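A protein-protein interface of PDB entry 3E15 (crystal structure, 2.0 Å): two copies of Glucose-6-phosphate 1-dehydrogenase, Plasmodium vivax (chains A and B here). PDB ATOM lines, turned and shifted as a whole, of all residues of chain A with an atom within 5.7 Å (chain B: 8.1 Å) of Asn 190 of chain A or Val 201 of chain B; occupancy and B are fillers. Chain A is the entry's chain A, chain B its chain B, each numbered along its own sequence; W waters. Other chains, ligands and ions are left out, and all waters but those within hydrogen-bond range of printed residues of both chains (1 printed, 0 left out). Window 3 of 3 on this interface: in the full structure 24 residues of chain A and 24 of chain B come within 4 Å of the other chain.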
ATOM      1  N   MET A 185      -0.915 -28.317  -1.074  1.00  0.00           N
ATOM      2  CA  MET A 185      -1.507 -28.270   0.224  1.00  0.00           C
ATOM      3  C   MET A 185      -2.932 -28.822   0.198  1.00  0.00           C
ATOM      4  O   MET A 185      -3.364 -29.435   1.163  1.00  0.00           O
ATOM      5  CB  MET A 185      -1.467 -26.832   0.761  1.00  0.00           C
ATOM      6  CG  MET A 185      -0.065 -26.298   0.973  1.00  0.00           C
ATOM      7  SD  MET A 185       0.898 -27.294   2.407  1.00  0.00           S
ATOM      8  CE  MET A 185      -0.142 -26.731   3.940  1.00  0.00           C
ATOM      9  N   TYR A 188      -2.174 -33.108  -1.912  1.00  0.00           N
ATOM     10  CA  TYR A 188      -1.095 -34.042  -1.624  1.00  0.00           C
ATOM     11  C   TYR A 188      -0.700 -34.064  -0.172  1.00  0.00           C
ATOM     12  O   TYR A 188      -0.297 -35.094   0.341  1.00  0.00           O
ATOM     13  CB  TYR A 188       0.124 -33.721  -2.458  1.00  0.00           C
ATOM     14  CG  TYR A 188      -0.049 -34.035  -3.913  1.00  0.00           C
ATOM     15  CD1 TYR A 188       0.181 -35.304  -4.398  1.00  0.00           C
ATOM     16  CD2 TYR A 188      -0.476 -33.050  -4.807  1.00  0.00           C
ATOM     17  CE1 TYR A 188       0.021 -35.594  -5.724  1.00  0.00           C
ATOM     18  CE2 TYR A 188      -0.647 -33.332  -6.130  1.00  0.00           C
ATOM     19  CZ  TYR A 188      -0.399 -34.601  -6.590  1.00  0.00           C
ATOM     20  OH  TYR A 188      -0.575 -34.873  -7.909  1.00  0.00           O
ATOM     21  N   GLN A 189      -0.782 -32.932   0.502  1.00  0.00           N
ATOM     22  CA  GLN A 189      -0.501 -32.917   1.920  1.00  0.00           C
ATOM     23  C   GLN A 189      -1.448 -33.908   2.638  1.00  0.00           C
ATOM     24  O   GLN A 189      -2.676 -33.911   2.419  1.00  0.00           O
ATOM     25  CB  GLN A 189      -0.589 -31.483   2.479  1.00  0.00           C
ATOM     26  CG  GLN A 189      -0.077 -31.313   3.879  1.00  0.00           C
ATOM     27  CD  GLN A 189       1.423 -31.505   3.994  1.00  0.00           C
ATOM     28  OE1 GLN A 189       2.200 -30.935   3.227  1.00  0.00           O
ATOM     29  NE2 GLN A 189       1.840 -32.304   4.970  1.00  0.00           N
ATOM     30  N   ASN A 190      -0.853 -34.787   3.445  1.00  0.00           N
ATOM     31  CA  ASN A 190      -1.596 -35.815   4.165  1.00  0.00           C
ATOM     32  C   ASN A 190      -2.301 -36.775   3.225  1.00  0.00           C
ATOM     33  O   ASN A 190      -3.222 -37.484   3.644  1.00  0.00           O
ATOM     34  CB  ASN A 190      -2.626 -35.195   5.114  1.00  0.00           C
ATOM     35  CG  ASN A 190      -1.989 -34.405   6.236  1.00  0.00           C
ATOM     36  OD1 ASN A 190      -0.933 -34.773   6.744  1.00  0.00           O
ATOM     37  ND2 ASN A 190      -2.632 -33.301   6.626  1.00  0.00           N
ATOM     38  N   SER A 191      -1.853 -36.807   1.968  1.00  0.00           N
ATOM     39  CA  SER A 191      -2.453 -37.656   0.928  1.00  0.00           C
ATOM     40  C   SER A 191      -3.963 -37.467   0.898  1.00  0.00           C
ATOM     41  O   SER A 191      -4.701 -38.412   0.676  1.00  0.00           O
ATOM     42  CB  SER A 191      -2.102 -39.128   1.156  1.00  0.00           C
ATOM     43  OG  SER A 191      -0.700 -39.324   1.049  1.00  0.00           O
ATOM     44  N   TYR A 192      -4.415 -36.230   1.088  1.00  0.00           N
ATOM     45  CA  TYR A 192      -5.848 -35.950   1.218  1.00  0.00           C
ATOM     46  C   TYR A 192      -6.616 -36.379  -0.043  1.00  0.00           C
ATOM     47  O   TYR A 192      -7.702 -36.960   0.047  1.00  0.00           O
ATOM     48  CB  TYR A 192      -6.087 -34.469   1.500  1.00  0.00           C
ATOM     49  CG  TYR A 192      -7.554 -34.080   1.705  1.00  0.00           C
ATOM     50  CD1 TYR A 192      -8.310 -34.603   2.767  1.00  0.00           C
ATOM     51  CD2 TYR A 192      -8.158 -33.163   0.870  1.00  0.00           C
ATOM     52  CE1 TYR A 192      -9.647 -34.215   2.953  1.00  0.00           C
ATOM     53  CE2 TYR A 192      -9.471 -32.775   1.043  1.00  0.00           C
ATOM     54  CZ  TYR A 192     -10.211 -33.298   2.073  1.00  0.00           C
ATOM     55  OH  TYR A 192     -11.515 -32.874   2.187  1.00  0.00           O
ATOM     56  N   TYR A 194      -4.603 -37.164  -3.443  1.00  0.00           N
ATOM     57  CA  TYR A 194      -3.644 -38.068  -4.108  1.00  0.00           C
ATOM     58  C   TYR A 194      -2.477 -38.420  -3.190  1.00  0.00           C
ATOM     59  O   TYR A 194      -2.154 -37.676  -2.290  1.00  0.00           O
ATOM     60  CB  TYR A 194      -3.096 -37.447  -5.392  1.00  0.00           C
ATOM     61  CG  TYR A 194      -4.178 -37.026  -6.340  1.00  0.00           C
ATOM     62  CD1 TYR A 194      -4.944 -37.976  -6.998  1.00  0.00           C
ATOM     63  CD2 TYR A 194      -4.453 -35.670  -6.577  1.00  0.00           C
ATOM     64  CE1 TYR A 194      -5.971 -37.594  -7.885  1.00  0.00           C
ATOM     65  CE2 TYR A 194      -5.481 -35.278  -7.451  1.00  0.00           C
ATOM     66  CZ  TYR A 194      -6.230 -36.253  -8.103  1.00  0.00           C
ATOM     67  OH  TYR A 194      -7.220 -35.899  -8.972  1.00  0.00           O
ATOM     68  N   GLU A 196       0.803 -38.715  -1.425  1.00  0.00           N
ATOM     69  CA  GLU A 196       1.967 -37.838  -1.255  1.00  0.00           C
ATOM     70  C   GLU A 196       3.299 -38.543  -1.575  1.00  0.00           C
ATOM     71  O   GLU A 196       4.253 -37.901  -2.023  1.00  0.00           O
ATOM     72  CB  GLU A 196       2.005 -37.289   0.167  1.00  0.00           C
ATOM     73  CG  GLU A 196       2.995 -36.173   0.349  1.00  0.00           C
ATOM     74  CD  GLU A 196       2.846 -35.465   1.673  1.00  0.00           C
ATOM     75  OE1 GLU A 196       2.217 -36.037   2.594  1.00  0.00           O
ATOM     76  OE2 GLU A 196       3.368 -34.328   1.799  1.00  0.00           O
ATOM     77  N   PHE B 180      -0.875 -19.229   4.929  1.00  0.00           N
ATOM     78  CA  PHE B 180      -0.560 -20.541   5.452  1.00  0.00           C
ATOM     79  C   PHE B 180       0.159 -21.470   4.439  1.00  0.00           C
ATOM     80  O   PHE B 180       1.180 -22.082   4.782  1.00  0.00           O
ATOM     81  CB  PHE B 180      -1.789 -21.234   6.059  1.00  0.00           C
ATOM     82  CG  PHE B 180      -1.453 -22.556   6.645  1.00  0.00           C
ATOM     83  CD1 PHE B 180      -0.677 -22.624   7.779  1.00  0.00           C
ATOM     84  CD2 PHE B 180      -1.839 -23.722   6.036  1.00  0.00           C
ATOM     85  CE1 PHE B 180      -0.328 -23.863   8.331  1.00  0.00           C
ATOM     86  CE2 PHE B 180      -1.479 -24.954   6.582  1.00  0.00           C
ATOM     87  CZ  PHE B 180      -0.722 -25.001   7.717  1.00  0.00           C
ATOM     88  N   PHE B 181      -0.360 -21.570   3.208  1.00  0.00           N
ATOM     89  CA  PHE B 181       0.261 -22.405   2.171  1.00  0.00           C
ATOM     90  C   PHE B 181       1.697 -21.933   1.870  1.00  0.00           C
ATOM     91  O   PHE B 181       2.614 -22.741   1.787  1.00  0.00           O
ATOM     92  CB  PHE B 181      -0.526 -22.365   0.837  1.00  0.00           C
ATOM     93  CG  PHE B 181      -1.932 -22.902   0.901  1.00  0.00           C
ATOM     94  CD1 PHE B 181      -2.414 -23.594   2.006  1.00  0.00           C
ATOM     95  CD2 PHE B 181      -2.778 -22.733  -0.192  1.00  0.00           C
ATOM     96  CE1 PHE B 181      -3.693 -24.096   2.019  1.00  0.00           C
ATOM     97  CE2 PHE B 181      -4.078 -23.239  -0.169  1.00  0.00           C
ATOM     98  CZ  PHE B 181      -4.526 -23.919   0.932  1.00  0.00           C
ATOM     99  N   TYR B 184       3.919 -22.503   4.979  1.00  0.00           N
ATOM    100  CA  TYR B 184       4.163 -23.936   5.175  1.00  0.00           C
ATOM    101  C   TYR B 184       5.162 -24.469   4.147  1.00  0.00           C
ATOM    102  O   TYR B 184       6.156 -25.136   4.486  1.00  0.00           O
ATOM    103  CB  TYR B 184       2.857 -24.773   5.132  1.00  0.00           C
ATOM    104  CG  TYR B 184       3.112 -26.154   5.681  1.00  0.00           C
ATOM    105  CD1 TYR B 184       2.930 -26.417   7.017  1.00  0.00           C
ATOM    106  CD2 TYR B 184       3.592 -27.179   4.870  1.00  0.00           C
ATOM    107  CE1 TYR B 184       3.181 -27.649   7.539  1.00  0.00           C
ATOM    108  CE2 TYR B 184       3.856 -28.428   5.399  1.00  0.00           C
ATOM    109  CZ  TYR B 184       3.645 -28.653   6.731  1.00  0.00           C
ATOM    110  OH  TYR B 184       3.897 -29.887   7.288  1.00  0.00           O
ATOM    111  N   TYR B 188       8.278 -25.066   6.458  1.00  0.00           N
ATOM    112  CA  TYR B 188       8.052 -26.290   7.246  1.00  0.00           C
ATOM    113  C   TYR B 188       8.187 -27.565   6.407  1.00  0.00           C
ATOM    114  O   TYR B 188       8.668 -28.593   6.905  1.00  0.00           O
ATOM    115  CB  TYR B 188       6.689 -26.252   7.916  1.00  0.00           C
ATOM    116  CG  TYR B 188       6.566 -25.231   9.040  1.00  0.00           C
ATOM    117  CD1 TYR B 188       6.864 -25.565  10.332  1.00  0.00           C
ATOM    118  CD2 TYR B 188       6.135 -23.910   8.782  1.00  0.00           C
ATOM    119  CE1 TYR B 188       6.760 -24.642  11.369  1.00  0.00           C
ATOM    120  CE2 TYR B 188       6.011 -22.987   9.811  1.00  0.00           C
ATOM    121  CZ  TYR B 188       6.337 -23.361  11.105  1.00  0.00           C
ATOM    122  OH  TYR B 188       6.216 -22.473  12.143  1.00  0.00           O
ATOM    123  N   GLN B 189       7.779 -27.496   5.148  1.00  0.00           N
ATOM    124  CA  GLN B 189       7.878 -28.630   4.249  1.00  0.00           C
ATOM    125  C   GLN B 189       9.362 -29.091   4.153  1.00  0.00           C
ATOM    126  O   GLN B 189      10.271 -28.290   3.888  1.00  0.00           O
ATOM    127  CB  GLN B 189       7.315 -28.257   2.865  1.00  0.00           C
ATOM    128  CG  GLN B 189       7.366 -29.364   1.793  1.00  0.00           C
ATOM    129  CD  GLN B 189       6.363 -30.482   2.052  1.00  0.00           C
ATOM    130  OE1 GLN B 189       5.604 -30.442   3.020  1.00  0.00           O
ATOM    131  NE2 GLN B 189       6.352 -31.481   1.174  1.00  0.00           N
ATOM    132  N   GLU B 196       9.285 -29.721  10.391  1.00  0.00           N
ATOM    133  CA  GLU B 196       7.989 -30.202   9.885  1.00  0.00           C
ATOM    134  C   GLU B 196       7.122 -30.770  11.012  1.00  0.00           C
ATOM    135  O   GLU B 196       5.908 -30.581  11.014  1.00  0.00           O
ATOM    136  CB  GLU B 196       8.224 -31.268   8.825  1.00  0.00           C
ATOM    137  CG  GLU B 196       7.201 -31.298   7.687  1.00  0.00           C
ATOM    138  CD  GLU B 196       7.525 -32.371   6.644  1.00  0.00           C
ATOM    139  OE1 GLU B 196       7.679 -32.039   5.439  1.00  0.00           O
ATOM    140  OE2 GLU B 196       7.622 -33.552   7.034  1.00  0.00           O
ATOM    141  N   SER B 197       7.745 -31.465  11.971  1.00  0.00           N
ATOM    142  CA  SER B 197       7.008 -32.139  13.043  1.00  0.00           C
ATOM    143  C   SER B 197       6.546 -31.197  14.126  1.00  0.00           C
ATOM    144  O   SER B 197       5.778 -31.590  14.999  1.00  0.00           O
ATOM    145  CB  SER B 197       7.874 -33.219  13.688  1.00  0.00           C
ATOM    146  OG  SER B 197       8.207 -34.193  12.722  1.00  0.00           O
ATOM    147  N   SER B 198       7.021 -29.956  14.092  1.00  0.00           N
ATOM    148  CA  SER B 198       6.616 -28.979  15.088  1.00  0.00           C
ATOM    149  C   SER B 198       5.187 -28.480  14.830  1.00  0.00           C
ATOM    150  O   SER B 198       4.675 -27.665  15.597  1.00  0.00           O
ATOM    151  CB  SER B 198       7.616 -27.812  15.148  1.00  0.00           C
ATOM    152  OG  SER B 198       7.545 -27.001  13.994  1.00  0.00           O
ATOM    153  N   ILE B 199       4.549 -29.003  13.770  1.00  0.00           N
ATOM    154  CA  ILE B 199       3.230 -28.549  13.308  1.00  0.00           C
ATOM    155  C   ILE B 199       2.384 -29.700  12.723  1.00  0.00           C
ATOM    156  O   ILE B 199       2.841 -30.447  11.847  1.00  0.00           O
ATOM    157  CB  ILE B 199       3.376 -27.468  12.210  1.00  0.00           C
ATOM    158  CG1 ILE B 199       3.873 -26.164  12.820  1.00  0.00           C
ATOM    159  CG2 ILE B 199       2.054 -27.225  11.511  1.00  0.00           C
ATOM    160  CD1 ILE B 199       3.204 -25.817  14.121  1.00  0.00           C
ATOM    161  N   LYS B 200       1.145 -29.822  13.197  1.00  0.00           N
ATOM    162  CA  LYS B 200       0.224 -30.851  12.703  1.00  0.00           C
ATOM    163  C   LYS B 200      -0.836 -30.233  11.800  1.00  0.00           C
ATOM    164  O   LYS B 200      -1.801 -29.647  12.289  1.00  0.00           O
ATOM    165  CB  LYS B 200      -0.452 -31.573  13.878  1.00  0.00           C
ATOM    166  N   VAL B 201      -0.649 -30.365  10.484  1.00  0.00           N
ATOM    167  CA  VAL B 201      -1.530 -29.726   9.494  1.00  0.00           C
ATOM    168  C   VAL B 201      -2.769 -30.578   9.241  1.00  0.00           C
ATOM    169  O   VAL B 201      -2.657 -31.790   9.056  1.00  0.00           O
ATOM    170  CB  VAL B 201      -0.824 -29.547   8.128  1.00  0.00           C
ATOM    171  CG1 VAL B 201      -1.800 -28.982   7.089  1.00  0.00           C
ATOM    172  CG2 VAL B 201       0.390 -28.667   8.267  1.00  0.00           C
ATOM    173  N   ALA B 202      -3.939 -29.934   9.212  1.00  0.00           N
ATOM    174  CA  ALA B 202      -5.202 -30.617   8.930  1.00  0.00           C
ATOM    175  C   ALA B 202      -5.761 -30.222   7.561  1.00  0.00           C
ATOM    176  O   ALA B 202      -5.780 -29.048   7.212  1.00  0.00           O
ATOM    177  CB  ALA B 202      -6.214 -30.301  10.022  1.00  0.00           C
ATOM    178  N   ASN B 203      -6.199 -31.225   6.793  1.00  0.00           N
ATOM    179  CA  ASN B 203      -7.177 -31.043   5.701  1.00  0.00           C
ATOM    180  C   ASN B 203      -8.598 -31.284   6.238  1.00  0.00           C
ATOM    181  O   ASN B 203      -9.595 -31.094   5.534  1.00  0.00           O
ATOM    182  CB  ASN B 203      -6.894 -32.030   4.556  1.00  0.00           C
ATOM    183  CG  ASN B 203      -5.993 -31.443   3.466  1.00  0.00           C
ATOM    184  OD1 ASN B 203      -6.455 -30.676   2.617  1.00  0.00           O
ATOM    185  ND2 ASN B 203      -4.710 -31.822   3.476  1.00  0.00           N
ATOM    186  N   THR B 207      -9.213 -28.525   8.725  1.00  0.00           N
ATOM    187  CA  THR B 207     -10.188 -27.618   9.331  1.00  0.00           C
ATOM    188  C   THR B 207     -10.390 -26.356   8.474  1.00  0.00           C
ATOM    189  O   THR B 207     -10.799 -26.451   7.304  1.00  0.00           O
ATOM    190  CB  THR B 207      -9.783 -27.225  10.775  1.00  0.00           C
ATOM    191  OG1 THR B 207      -8.382 -26.890  10.818  1.00  0.00           O
ATOM    192  CG2 THR B 207     -10.075 -28.380  11.756  1.00  0.00           C
ATOM    193  N   ASN B 212      -5.351 -23.473  10.973  1.00  0.00           N
ATOM    194  CA  ASN B 212      -3.981 -23.840  10.616  1.00  0.00           C
ATOM    195  C   ASN B 212      -2.977 -22.673  10.811  1.00  0.00           C
ATOM    196  O   ASN B 212      -1.888 -22.867  11.341  1.00  0.00           O
ATOM    197  CB  ASN B 212      -3.922 -24.369   9.179  1.00  0.00           C
ATOM    198  CG  ASN B 212      -4.500 -25.772   9.035  1.00  0.00           C
ATOM    199  OD1 ASN B 212      -4.488 -26.567   9.972  1.00  0.00           O
ATOM    200  ND2 ASN B 212      -4.962 -26.092   7.842  1.00  0.00           N
ATOM    201  N   LEU B 215      -1.483 -22.279  14.107  1.00  0.00           N
ATOM    202  CA  LEU B 215      -0.453 -23.233  14.499  1.00  0.00           C
ATOM    203  C   LEU B 215       0.954 -22.673  14.305  1.00  0.00           C
ATOM    204  O   LEU B 215       1.886 -23.181  14.895  1.00  0.00           O
ATOM    205  CB  LEU B 215      -0.593 -24.528  13.717  1.00  0.00           C
ATOM    206  CG  LEU B 215      -1.856 -25.307  14.060  1.00  0.00           C
ATOM    207  CD1 LEU B 215      -1.948 -26.547  13.244  1.00  0.00           C
ATOM    208  CD2 LEU B 215      -1.880 -25.619  15.562  1.00  0.00           C
ATOM    209  N   LEU B 216       1.089 -21.633  13.482  1.00  0.00           N
ATOM    210  CA  LEU B 216       2.395 -21.003  13.213  1.00  0.00           C
ATOM    211  C   LEU B 216       2.885 -20.178  14.414  1.00  0.00           C
ATOM    212  O   LEU B 216       2.252 -19.210  14.808  1.00  0.00           O
ATOM    213  CB  LEU B 216       2.289 -20.090  11.998  1.00  0.00           C
ATOM    214  CG  LEU B 216       1.830 -20.732  10.697  1.00  0.00           C
ATOM    215  CD1 LEU B 216       1.635 -19.669   9.586  1.00  0.00           C
ATOM    216  CD2 LEU B 216       2.805 -21.793  10.267  1.00  0.00           C
HETATM  217  O   HOH W   1      -3.012 -28.871   3.875  1.00  0.00           O
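The backbone carbonyl oxygen (O) of Tyr 184 of chain B sits at hydrogen-bond distance from the backbone NH (N) of Gln 189 of chain B, at 2.9 Å.
The backbone NH (N) of Asn 190 of chain A sits at hydrogen-bond distance from the side-chain carboxylate (OE1) of Glu 196 of chain A, 3.4 Å away.
Gln 189 of chain B touches its own counterpart, Gln 189 of chain A.
Of the 9 pairs that touch across the chains among the printed residues, 1 has its exchanged pair printed and touching as well.
Among the printed residues, pairs that only touch across the chains: Tyr 192 of chain A with Asn 203 of chain B (3.4 Å), Met 185 of chain A with Phe 180 of chain B (3.5 Å), Met 185 of chain A with Asn 203 of chain B (3.6 Å), Met 185 of chain A with Phe 181 of chain B (3.6 Å), Met 185 of chain A with Tyr 184 of chain B (3.7 Å) and Gln 189 of chain A with Tyr 184 of chain B (3.7 Å).
The backbone carbonyl oxygen (O) of Gln 189 of chain A sits at hydrogen-bond distance from the side-chain amide nitrogen (ND2) of Asn 203 of chain B (3.1 Å).
OE1 of Gln 189 of chain A lies close to OE1 of Gln 189 of chain B, at 3.4 Å.
The backbone carbonyl oxygen of Val 201 of chain B sits at hydrogen-bond distance from the side-chain amide nitrogen of Asn 190 of chain A (2.9 Å).
Asn 190 of chain A touches just one residue of chain B: Val 201 (2.9 Å).
No residue of chain B comes within 4 Å of Ser 191 of chain A.
Printed residues of chain B within 4 Å of Met 185 of chain A: Phe 180, Phe 181, Tyr 184 and Asn 203.
Printed residues of chain A within 4 Å of Tyr 184 of chain B: Met 185 and Gln 189.
Glu 196 of chain B touches none of the printed residues of chain A.
Lys 200 of chain B touches none of the printed residues of chain A.
The nearest residue of chain B that does not touch Asn 190 of chain A is Asn 203 of chain B (4.1 Å).
Of the 8 printed residues of chain A, 4 touch a printed residue of chain B.
Hydrophobic or aromatic side chains of chain A within 4 Å of the printed part of chain B: Met 185 and Tyr 192.
Printed residues of chain B that touch a printed residue of chain A: Phe 180, Phe 181, Tyr 184, Gln 189, Val 201 and Asn 203.
Among the printed residues, no Asp or Glu carboxylate lies within 4 Å of a Lys or Arg side-chain nitrogen of the other chain.
Water W1 lies within hydrogen-bond range of O of Met 185 of chain A (2.8 Å) and ND2 of Asn 203 of chain B (3.4 Å).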
